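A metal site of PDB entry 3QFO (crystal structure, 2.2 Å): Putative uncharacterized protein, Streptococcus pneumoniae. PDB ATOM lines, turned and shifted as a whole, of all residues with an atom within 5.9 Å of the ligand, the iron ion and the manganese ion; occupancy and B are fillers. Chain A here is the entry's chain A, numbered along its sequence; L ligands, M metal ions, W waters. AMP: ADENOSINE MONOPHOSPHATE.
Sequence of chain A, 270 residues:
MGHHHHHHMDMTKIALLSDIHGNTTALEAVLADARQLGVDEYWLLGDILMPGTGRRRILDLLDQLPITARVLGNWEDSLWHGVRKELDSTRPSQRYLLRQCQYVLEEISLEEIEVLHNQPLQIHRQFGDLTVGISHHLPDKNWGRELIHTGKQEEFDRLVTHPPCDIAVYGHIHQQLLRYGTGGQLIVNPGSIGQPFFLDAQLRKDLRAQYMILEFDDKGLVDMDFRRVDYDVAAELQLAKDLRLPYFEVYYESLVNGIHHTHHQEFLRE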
ATOM      1  N   ASP A  19      -4.741  17.761 -12.929  1.00  0.00           N
ATOM      2  CA  ASP A  19      -3.592  18.280 -12.173  1.00  0.00           C
ATOM      3  C   ASP A  19      -3.842  18.184 -10.657  1.00  0.00           C
ATOM      4  O   ASP A  19      -3.745  19.176  -9.919  1.00  0.00           O
ATOM      5  CB  ASP A  19      -3.292  19.716 -12.619  1.00  0.00           C
ATOM      6  CG  ASP A  19      -2.868  19.796 -14.089  1.00  0.00           C
ATOM      7  OD1 ASP A  19      -3.645  20.342 -14.925  1.00  0.00           O
ATOM      8  OD2 ASP A  19      -1.755  19.287 -14.394  1.00  0.00           O
ATOM      9  N   HIS A  21      -1.989  16.129  -8.742  1.00  0.00           N
ATOM     10  CA  HIS A  21      -0.618  16.135  -8.241  1.00  0.00           C
ATOM     11  C   HIS A  21      -0.489  15.578  -6.830  1.00  0.00           C
ATOM     12  O   HIS A  21       0.245  16.121  -6.009  1.00  0.00           O
ATOM     13  CB  HIS A  21      -0.029  17.544  -8.314  1.00  0.00           C
ATOM     14  CG  HIS A  21       0.347  17.970  -9.704  1.00  0.00           C
ATOM     15  ND1 HIS A  21       1.547  17.622 -10.288  1.00  0.00           N
ATOM     16  CD2 HIS A  21      -0.334  18.699 -10.621  1.00  0.00           C
ATOM     17  CE1 HIS A  21       1.606  18.137 -11.502  1.00  0.00           C
ATOM     18  NE2 HIS A  21       0.474  18.781 -11.734  1.00  0.00           N
ATOM     19  N   GLY A  46      -5.233  14.281 -16.348  1.00  0.00           N
ATOM     20  CA  GLY A  46      -3.853  13.861 -16.051  1.00  0.00           C
ATOM     21  C   GLY A  46      -3.096  14.710 -15.035  1.00  0.00           C
ATOM     22  O   GLY A  46      -3.633  15.710 -14.499  1.00  0.00           O
ATOM     23  N   ASP A  47      -1.841  14.326 -14.801  1.00  0.00           N
ATOM     24  CA  ASP A  47      -1.029  14.785 -13.661  1.00  0.00           C
ATOM     25  C   ASP A  47      -1.718  14.406 -12.353  1.00  0.00           C
ATOM     26  O   ASP A  47      -2.175  15.239 -11.572  1.00  0.00           O
ATOM     27  CB  ASP A  47      -0.657  16.271 -13.755  1.00  0.00           C
ATOM     28  CG  ASP A  47       0.359  16.555 -14.853  1.00  0.00           C
ATOM     29  OD1 ASP A  47       0.771  15.592 -15.550  1.00  0.00           O
ATOM     30  OD2 ASP A  47       0.747  17.727 -15.058  1.00  0.00           O
ATOM     31  N   GLY A  73      -1.061  12.790 -18.744  1.00  0.00           N
ATOM     32  CA  GLY A  73      -0.310  13.991 -18.380  1.00  0.00           C
ATOM     33  C   GLY A  73       1.190  13.737 -18.403  1.00  0.00           C
ATOM     34  O   GLY A  73       1.626  12.591 -18.368  1.00  0.00           O
ATOM     35  N   ASN A  74       1.988  14.806 -18.452  1.00  0.00           N
ATOM     36  CA  ASN A  74       3.449  14.651 -18.466  1.00  0.00           C
ATOM     37  C   ASN A  74       4.034  14.067 -17.168  1.00  0.00           C
ATOM     38  O   ASN A  74       5.116  13.467 -17.199  1.00  0.00           O
ATOM     39  CB  ASN A  74       4.112  15.974 -18.788  1.00  0.00           C
ATOM     40  CG  ASN A  74       3.619  17.098 -17.884  1.00  0.00           C
ATOM     41  OD1 ASN A  74       2.424  17.222 -17.645  1.00  0.00           O
ATOM     42  ND2 ASN A  74       4.541  17.877 -17.357  1.00  0.00           N
ATOM     43  N   TRP A  75       3.338  14.244 -16.039  1.00  0.00           N
ATOM     44  CA  TRP A  75       3.785  13.659 -14.774  1.00  0.00           C
ATOM     45  C   TRP A  75       3.600  12.131 -14.702  1.00  0.00           C
ATOM     46  O   TRP A  75       4.292  11.467 -13.934  1.00  0.00           O
ATOM     47  CB  TRP A  75       3.180  14.368 -13.556  1.00  0.00           C
ATOM     48  CG  TRP A  75       3.857  15.693 -13.256  1.00  0.00           C
ATOM     49  CD1 TRP A  75       3.796  16.828 -14.013  1.00  0.00           C
ATOM     50  CD2 TRP A  75       4.686  16.018 -12.139  1.00  0.00           C
ATOM     51  NE1 TRP A  75       4.551  17.829 -13.456  1.00  0.00           N
ATOM     52  CE2 TRP A  75       5.092  17.362 -12.287  1.00  0.00           C
ATOM     53  CE3 TRP A  75       5.140  15.304 -11.017  1.00  0.00           C
ATOM     54  CZ2 TRP A  75       5.927  18.012 -11.363  1.00  0.00           C
ATOM     55  CZ3 TRP A  75       5.985  15.950 -10.092  1.00  0.00           C
ATOM     56  CH2 TRP A  75       6.358  17.292 -10.269  1.00  0.00           C
ATOM     57  N   HIS A 136      -4.111  16.620 -22.314  1.00  0.00           N
ATOM     58  CA  HIS A 136      -3.475  17.273 -21.163  1.00  0.00           C
ATOM     59  C   HIS A 136      -2.991  18.661 -21.551  1.00  0.00           C
ATOM     60  O   HIS A 136      -3.270  19.640 -20.871  1.00  0.00           O
ATOM     61  CB  HIS A 136      -2.306  16.460 -20.602  1.00  0.00           C
ATOM     62  CG  HIS A 136      -1.701  17.052 -19.356  1.00  0.00           C
ATOM     63  ND1 HIS A 136      -2.390  17.096 -18.161  1.00  0.00           N
ATOM     64  CD2 HIS A 136      -0.493  17.625 -19.125  1.00  0.00           C
ATOM     65  CE1 HIS A 136      -1.625  17.665 -17.236  1.00  0.00           C
ATOM     66  NE2 HIS A 136      -0.468  17.981 -17.799  1.00  0.00           N
ATOM     67  N   ASN A 142       2.323  16.411 -24.338  1.00  0.00           N
ATOM     68  CA  ASN A 142       1.683  16.684 -23.039  1.00  0.00           C
ATOM     69  C   ASN A 142       2.542  17.523 -22.067  1.00  0.00           C
ATOM     70  O   ASN A 142       2.240  17.615 -20.876  1.00  0.00           O
ATOM     71  CB  ASN A 142       1.209  15.385 -22.384  1.00  0.00           C
ATOM     72  CG  ASN A 142       2.352  14.497 -21.951  1.00  0.00           C
ATOM     73  OD1 ASN A 142       3.515  14.882 -21.974  1.00  0.00           O
ATOM     74  ND2 ASN A 142       2.027  13.293 -21.523  1.00  0.00           N
ATOM     75  N   ARG A 145       5.229  24.721 -22.764  1.00  0.00           N
ATOM     76  CA  ARG A 145       4.664  26.007 -22.378  1.00  0.00           C
ATOM     77  C   ARG A 145       3.910  26.652 -23.524  1.00  0.00           C
ATOM     78  O   ARG A 145       3.563  27.837 -23.435  1.00  0.00           O
ATOM     79  CB  ARG A 145       5.765  26.969 -21.945  1.00  0.00           C
ATOM     80  CG  ARG A 145       6.570  26.559 -20.732  1.00  0.00           C
ATOM     81  CD  ARG A 145       5.705  26.311 -19.496  1.00  0.00           C
ATOM     82  NE  ARG A 145       6.446  26.658 -18.276  1.00  0.00           N
ATOM     83  CZ  ARG A 145       6.441  25.934 -17.168  1.00  0.00           C
ATOM     84  NH1 ARG A 145       7.158  26.335 -16.120  1.00  0.00           N
ATOM     85  NH2 ARG A 145       5.747  24.799 -17.107  1.00  0.00           N
ATOM     86  N   ILE A 148       0.346  28.412 -22.508  1.00  0.00           N
ATOM     87  CA  ILE A 148       0.257  29.295 -21.355  1.00  0.00           C
ATOM     88  C   ILE A 148      -0.728  30.449 -21.627  1.00  0.00           C
ATOM     89  O   ILE A 148      -1.192  30.622 -22.771  1.00  0.00           O
ATOM     90  CB  ILE A 148       1.636  29.870 -20.921  1.00  0.00           C
ATOM     91  CG1 ILE A 148       2.315  30.644 -22.065  1.00  0.00           C
ATOM     92  CG2 ILE A 148       2.507  28.748 -20.348  1.00  0.00           C
ATOM     93  CD1 ILE A 148       3.615  31.384 -21.634  1.00  0.00           C
ATOM     94  N   HIS A 149      -1.023  31.229 -20.597  1.00  0.00           N
ATOM     95  CA  HIS A 149      -1.999  32.314 -20.688  1.00  0.00           C
ATOM     96  C   HIS A 149      -1.730  33.280 -21.852  1.00  0.00           C
ATOM     97  O   HIS A 149      -2.659  33.811 -22.439  1.00  0.00           O
ATOM     98  CB  HIS A 149      -2.147  33.057 -19.336  1.00  0.00           C
ATOM     99  CG  HIS A 149      -0.970  33.900 -18.951  1.00  0.00           C
ATOM    100  ND1 HIS A 149       0.328  33.432 -18.984  1.00  0.00           N
ATOM    101  CD2 HIS A 149      -0.891  35.181 -18.519  1.00  0.00           C
ATOM    102  CE1 HIS A 149       1.153  34.393 -18.607  1.00  0.00           C
ATOM    103  NE2 HIS A 149       0.439  35.466 -18.316  1.00  0.00           N
ATOM    104  N   THR A 150      -0.455  33.474 -22.194  1.00  0.00           N
ATOM    105  CA  THR A 150      -0.079  34.380 -23.283  1.00  0.00           C
ATOM    106  C   THR A 150       0.378  33.644 -24.543  1.00  0.00           C
ATOM    107  O   THR A 150       1.036  34.233 -25.409  1.00  0.00           O
ATOM    108  CB  THR A 150       1.021  35.370 -22.839  1.00  0.00           C
ATOM    109  OG1 THR A 150       2.088  34.657 -22.217  1.00  0.00           O
ATOM    110  CG2 THR A 150       0.473  36.393 -21.851  1.00  0.00           C
ATOM    111  N   HIS A 172      -2.852  21.156 -17.606  1.00  0.00           N
ATOM    112  CA  HIS A 172      -1.404  21.421 -17.699  1.00  0.00           C
ATOM    113  C   HIS A 172      -0.920  22.796 -17.214  1.00  0.00           C
ATOM    114  O   HIS A 172       0.135  22.897 -16.596  1.00  0.00           O
ATOM    115  CB  HIS A 172      -0.877  21.126 -19.102  1.00  0.00           C
ATOM    116  CG  HIS A 172       0.603  21.210 -19.232  1.00  0.00           C
ATOM    117  ND1 HIS A 172       1.471  20.383 -18.531  1.00  0.00           N
ATOM    118  CD2 HIS A 172       1.383  22.054 -19.961  1.00  0.00           C
ATOM    119  CE1 HIS A 172       2.717  20.705 -18.847  1.00  0.00           C
ATOM    120  NE2 HIS A 172       2.690  21.699 -19.703  1.00  0.00           N
ATOM    121  N   ILE A 173      -1.661  23.860 -17.519  1.00  0.00           N
ATOM    122  CA  ILE A 173      -1.195  25.188 -17.122  1.00  0.00           C
ATOM    123  C   ILE A 173      -1.645  25.608 -15.718  1.00  0.00           C
ATOM    124  O   ILE A 173      -1.163  26.617 -15.199  1.00  0.00           O
ATOM    125  CB  ILE A 173      -1.549  26.277 -18.166  1.00  0.00           C
ATOM    126  CG1 ILE A 173      -3.073  26.465 -18.276  1.00  0.00           C
ATOM    127  CG2 ILE A 173      -0.892  25.962 -19.515  1.00  0.00           C
ATOM    128  CD1 ILE A 173      -3.484  27.780 -18.935  1.00  0.00           C
ATOM    129  N   HIS A 174      -2.550  24.832 -15.108  1.00  0.00           N
ATOM    130  CA  HIS A 174      -2.958  25.043 -13.721  1.00  0.00           C
ATOM    131  C   HIS A 174      -3.698  26.377 -13.559  1.00  0.00           C
ATOM    132  O   HIS A 174      -3.634  27.030 -12.507  1.00  0.00           O
ATOM    133  CB  HIS A 174      -1.737  24.978 -12.772  1.00  0.00           C
ATOM    134  CG  HIS A 174      -1.147  23.603 -12.619  1.00  0.00           C
ATOM    135  ND1 HIS A 174      -0.637  23.140 -11.415  1.00  0.00           N
ATOM    136  CD2 HIS A 174      -1.012  22.578 -13.500  1.00  0.00           C
ATOM    137  CE1 HIS A 174      -0.214  21.898 -11.568  1.00  0.00           C
ATOM    138  NE2 HIS A 174      -0.411  21.532 -12.819  1.00  0.00           N
ATOM    139  N   GLN A 175      -4.387  26.782 -14.624  1.00  0.00           N
ATOM    140  CA  GLN A 175      -5.215  27.988 -14.624  1.00  0.00           C
ATOM    141  C   GLN A 175      -6.560  27.696 -15.293  1.00  0.00           C
ATOM    142  O   GLN A 175      -6.629  26.965 -16.267  1.00  0.00           O
ATOM    143  CB  GLN A 175      -4.536  29.121 -15.405  1.00  0.00           C
ATOM    144  CG  GLN A 175      -3.169  29.597 -14.894  1.00  0.00           C
ATOM    145  CD  GLN A 175      -2.807  30.912 -15.551  1.00  0.00           C
ATOM    146  OE1 GLN A 175      -2.246  30.924 -16.650  1.00  0.00           O
ATOM    147  NE2 GLN A 175      -3.220  32.025 -14.929  1.00  0.00           N
ATOM    148  N   SER A 192      -6.258  23.583 -11.765  1.00  0.00           N
ATOM    149  CA  SER A 192      -5.623  22.480 -11.032  1.00  0.00           C
ATOM    150  C   SER A 192      -6.302  22.219  -9.688  1.00  0.00           C
ATOM    151  O   SER A 192      -6.533  23.125  -8.907  1.00  0.00           O
ATOM    152  CB  SER A 192      -4.135  22.826 -10.803  1.00  0.00           C
ATOM    153  OG  SER A 192      -3.493  21.865  -9.989  1.00  0.00           O
ATOM    154  N   GLN A 195      -2.608  22.027  -7.177  1.00  0.00           N
ATOM    155  CA  GLN A 195      -1.526  23.000  -7.294  1.00  0.00           C
ATOM    156  C   GLN A 195      -1.986  24.239  -8.099  1.00  0.00           C
ATOM    157  O   GLN A 195      -1.354  24.573  -9.105  1.00  0.00           O
ATOM    158  CB  GLN A 195      -0.297  22.405  -8.008  1.00  0.00           C
ATOM    159  CG  GLN A 195       0.353  21.136  -7.394  1.00  0.00           C
ATOM    160  CD  GLN A 195       1.220  21.449  -6.178  1.00  0.00           C
ATOM    161  OE1 GLN A 195       2.451  21.516  -6.285  1.00  0.00           O
ATOM    162  NE2 GLN A 195       0.582  21.671  -5.034  1.00  0.00           N
ATOM    163  N   PHE A 197      -2.478  27.758  -9.845  1.00  0.00           N
ATOM    164  CA  PHE A 197      -1.382  28.624 -10.225  1.00  0.00           C
ATOM    165  C   PHE A 197      -1.867  29.996 -10.623  1.00  0.00           C
ATOM    166  O   PHE A 197      -2.751  30.143 -11.472  1.00  0.00           O
ATOM    167  CB  PHE A 197      -0.525  27.996 -11.330  1.00  0.00           C
ATOM    168  CG  PHE A 197       0.622  28.856 -11.781  1.00  0.00           C
ATOM    169  CD1 PHE A 197       1.722  29.084 -10.938  1.00  0.00           C
ATOM    170  CD2 PHE A 197       0.604  29.457 -13.042  1.00  0.00           C
ATOM    171  CE1 PHE A 197       2.794  29.912 -11.343  1.00  0.00           C
ATOM    172  CE2 PHE A 197       1.673  30.277 -13.465  1.00  0.00           C
ATOM    173  CZ  PHE A 197       2.763  30.504 -12.609  1.00  0.00           C
ATOM    174  N   LEU A 199      -0.391  34.040 -11.465  1.00  0.00           N
ATOM    175  CA  LEU A 199       0.679  35.011 -11.667  1.00  0.00           C
ATOM    176  C   LEU A 199       0.362  36.304 -10.916  1.00  0.00           C
ATOM    177  O   LEU A 199       1.255  37.097 -10.621  1.00  0.00           O
ATOM    178  CB  LEU A 199       0.925  35.307 -13.157  1.00  0.00           C
ATOM    179  CG  LEU A 199       1.683  34.245 -13.953  1.00  0.00           C
ATOM    180  CD1 LEU A 199       0.702  33.297 -14.586  1.00  0.00           C
ATOM    181  CD2 LEU A 199       2.521  34.867 -15.057  1.00  0.00           C
ATOM    182  N   HIS A 260       5.767  28.361  -6.994  1.00  0.00           N
ATOM    183  CA  HIS A 260       6.198  27.057  -7.516  1.00  0.00           C
ATOM    184  C   HIS A 260       7.701  26.998  -7.808  1.00  0.00           C
ATOM    185  O   HIS A 260       8.216  27.782  -8.614  1.00  0.00           O
ATOM    186  CB  HIS A 260       5.364  26.657  -8.744  1.00  0.00           C
ATOM    187  CG  HIS A 260       3.902  26.412  -8.450  1.00  0.00           C
ATOM    188  ND1 HIS A 260       2.965  26.261  -9.449  1.00  0.00           N
ATOM    189  CD2 HIS A 260       3.239  26.291  -7.288  1.00  0.00           C
ATOM    190  CE1 HIS A 260       1.781  26.050  -8.905  1.00  0.00           C
ATOM    191  NE2 HIS A 260       1.917  26.060  -7.592  1.00  0.00           N
HETATM  192  P   AMP L   1       3.201  20.587 -14.868  1.00  0.00           P
HETATM  193  O1P AMP L   1       2.953  19.803 -16.132  1.00  0.00           O
HETATM  194  O2P AMP L   1       2.246  20.295 -13.743  1.00  0.00           O
HETATM  195  O3P AMP L   1       4.642  20.491 -14.455  1.00  0.00           O
HETATM  196  O5' AMP L   1       2.988  22.131 -15.292  1.00  0.00           O
HETATM  197  C5' AMP L   1       2.212  23.053 -14.534  1.00  0.00           C
HETATM  198  C4' AMP L   1       3.084  24.175 -13.980  1.00  0.00           C
HETATM  199  O4' AMP L   1       3.634  25.004 -15.007  1.00  0.00           O
HETATM  200  C3' AMP L   1       2.278  25.161 -13.134  1.00  0.00           C
HETATM  201  O3' AMP L   1       2.064  24.686 -11.803  1.00  0.00           O
HETATM  202  C2' AMP L   1       3.160  26.379 -13.126  1.00  0.00           C
HETATM  203  O2' AMP L   1       4.107  26.286 -12.047  1.00  0.00           O
HETATM  204  C1' AMP L   1       3.853  26.318 -14.478  1.00  0.00           C
HETATM  205  N9  AMP L   1       3.258  27.383 -15.333  1.00  0.00           N
HETATM  206  C8  AMP L   1       2.047  27.350 -15.945  1.00  0.00           C
HETATM  207  N7  AMP L   1       1.823  28.506 -16.631  1.00  0.00           N
HETATM  208  C5  AMP L   1       2.904  29.291 -16.460  1.00  0.00           C
HETATM  209  C6  AMP L   1       3.313  30.646 -16.899  1.00  0.00           C
HETATM  210  N6  AMP L   1       2.501  31.391 -17.683  1.00  0.00           N
HETATM  211  N1  AMP L   1       4.526  31.109 -16.480  1.00  0.00           N
HETATM  212  C2  AMP L   1       5.348  30.389 -15.686  1.00  0.00           C
HETATM  213  N3  AMP L   1       5.029  29.140 -15.251  1.00  0.00           N
HETATM  214  C4  AMP L   1       3.846  28.550 -15.599  1.00  0.00           C
HETATM  215 FE    FE M   1       0.222  19.630 -13.766  1.00  0.00          FE
HETATM  216 MN    MN M   2       1.230  18.887 -16.852  1.00  0.00          MN
HETATM  217  O   HOH W   1       3.148  21.569 -11.119  1.00  0.00           O
HETATM  218  O   HOH W   2      -0.066  29.994 -17.982  1.00  0.00           O
HETATM  219  O   HOH W   3       0.787  20.389 -15.633  1.00  0.00           O
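ND1 of His 260 is in hydrogen-bond range of O2' of the ligand, 2.8 Å away.
An oxygen (O3P) of the ligand is in hydrogen-bond range of the indole nitrogen (NE1) of Trp 75.
NH2 of Arg 145 sits at hydrogen-bond distance from O4' of the ligand, at 3.0 Å.
A ring nitrogen (ND1) of His 149 sits at hydrogen-bond distance from a nitrogen (N6) of the ligand (3.3 Å).
OD1 of Asp 19 sits at hydrogen-bond distance from N of His 172 (2.9 Å).
N of Asp 19 lies within hydrogen-bond range of O of Gly 46, at 2.8 Å.
The backbone carbonyl oxygen (O) of Asp 19 is in hydrogen-bond range of the side-chain hydroxyl (OG) of Ser 192, 2.7 Å away.
OD1 of Asp 47 lies within hydrogen-bond range of N of Trp 75.
The backbone NH (N) of Asn 74 sits close to the side-chain amide nitrogen (ND2) of Asn 142 (3.4 Å).
The backbone carbonyl oxygen (O) of His 174 lies within hydrogen-bond range of the backbone NH (N) of Phe 197 (3.0 Å).
A ring nitrogen (ND1) of His 174 is in hydrogen-bond range of the backbone carbonyl oxygen (O) of Gln 195, 2.8 Å away.
ND1 of His 174 lies within hydrogen-bond range of OG of Ser 192, at 3.4 Å.
Merely in contact with the ligand: Ile 173 (3.4 Å), Phe 197 (3.4 Å) and Ile 148 (3.7 Å).
12 residues have an atom within 4 Å of the ligand: His 21, Asp 47, Asn 74, Trp 75, Arg 145, Ile 148, His 149, His 172, Ile 173, His 174, Phe 197 and His 260.
Five residues have an atom within 4 Å of the manganese ion: Asp 19, Asp 47, Asn 74, His 136 and His 172.
The nearest printed residue that does not touch the manganese ion is Asn 142 (4.3 Å).
Water W3 binds the iron ion (2.1 Å).
OD2 of Asp 19 binds the iron ion, at 2.1 Å.
O2P of the ligand binds the iron ion (2.1 Å).
A ring nitrogen (NE2) of His 21 binds the iron ion (2.2 Å).
NE2 of His 174 binds the iron ion (2.2 Å).
The iron ion is bound by OD2 of Asp 47 (2.4 Å).
The iron ion has six donor atoms within binding distance.
The manganese ion is bound by water W3 (2.0 Å), O1P of the ligand (2.1 Å), NE2 of His 136 (2.1 Å), OD2 of Asp 47 (2.2 Å), OD1 of Asn 74 (2.2 Å) and ND1 of His 172 (2.3 Å).
Water W3 bridges O of His 172 (2.8 Å) and O5' of the ligand (2.8 Å).
Water W2 lies within hydrogen-bond range of the side-chain amide oxygen (OE1) of Gln 175 (2.7 Å), a nitrogen (N7) of the ligand (2.8 Å) and the backbone NH (N) of His 149 (3.0 Å).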
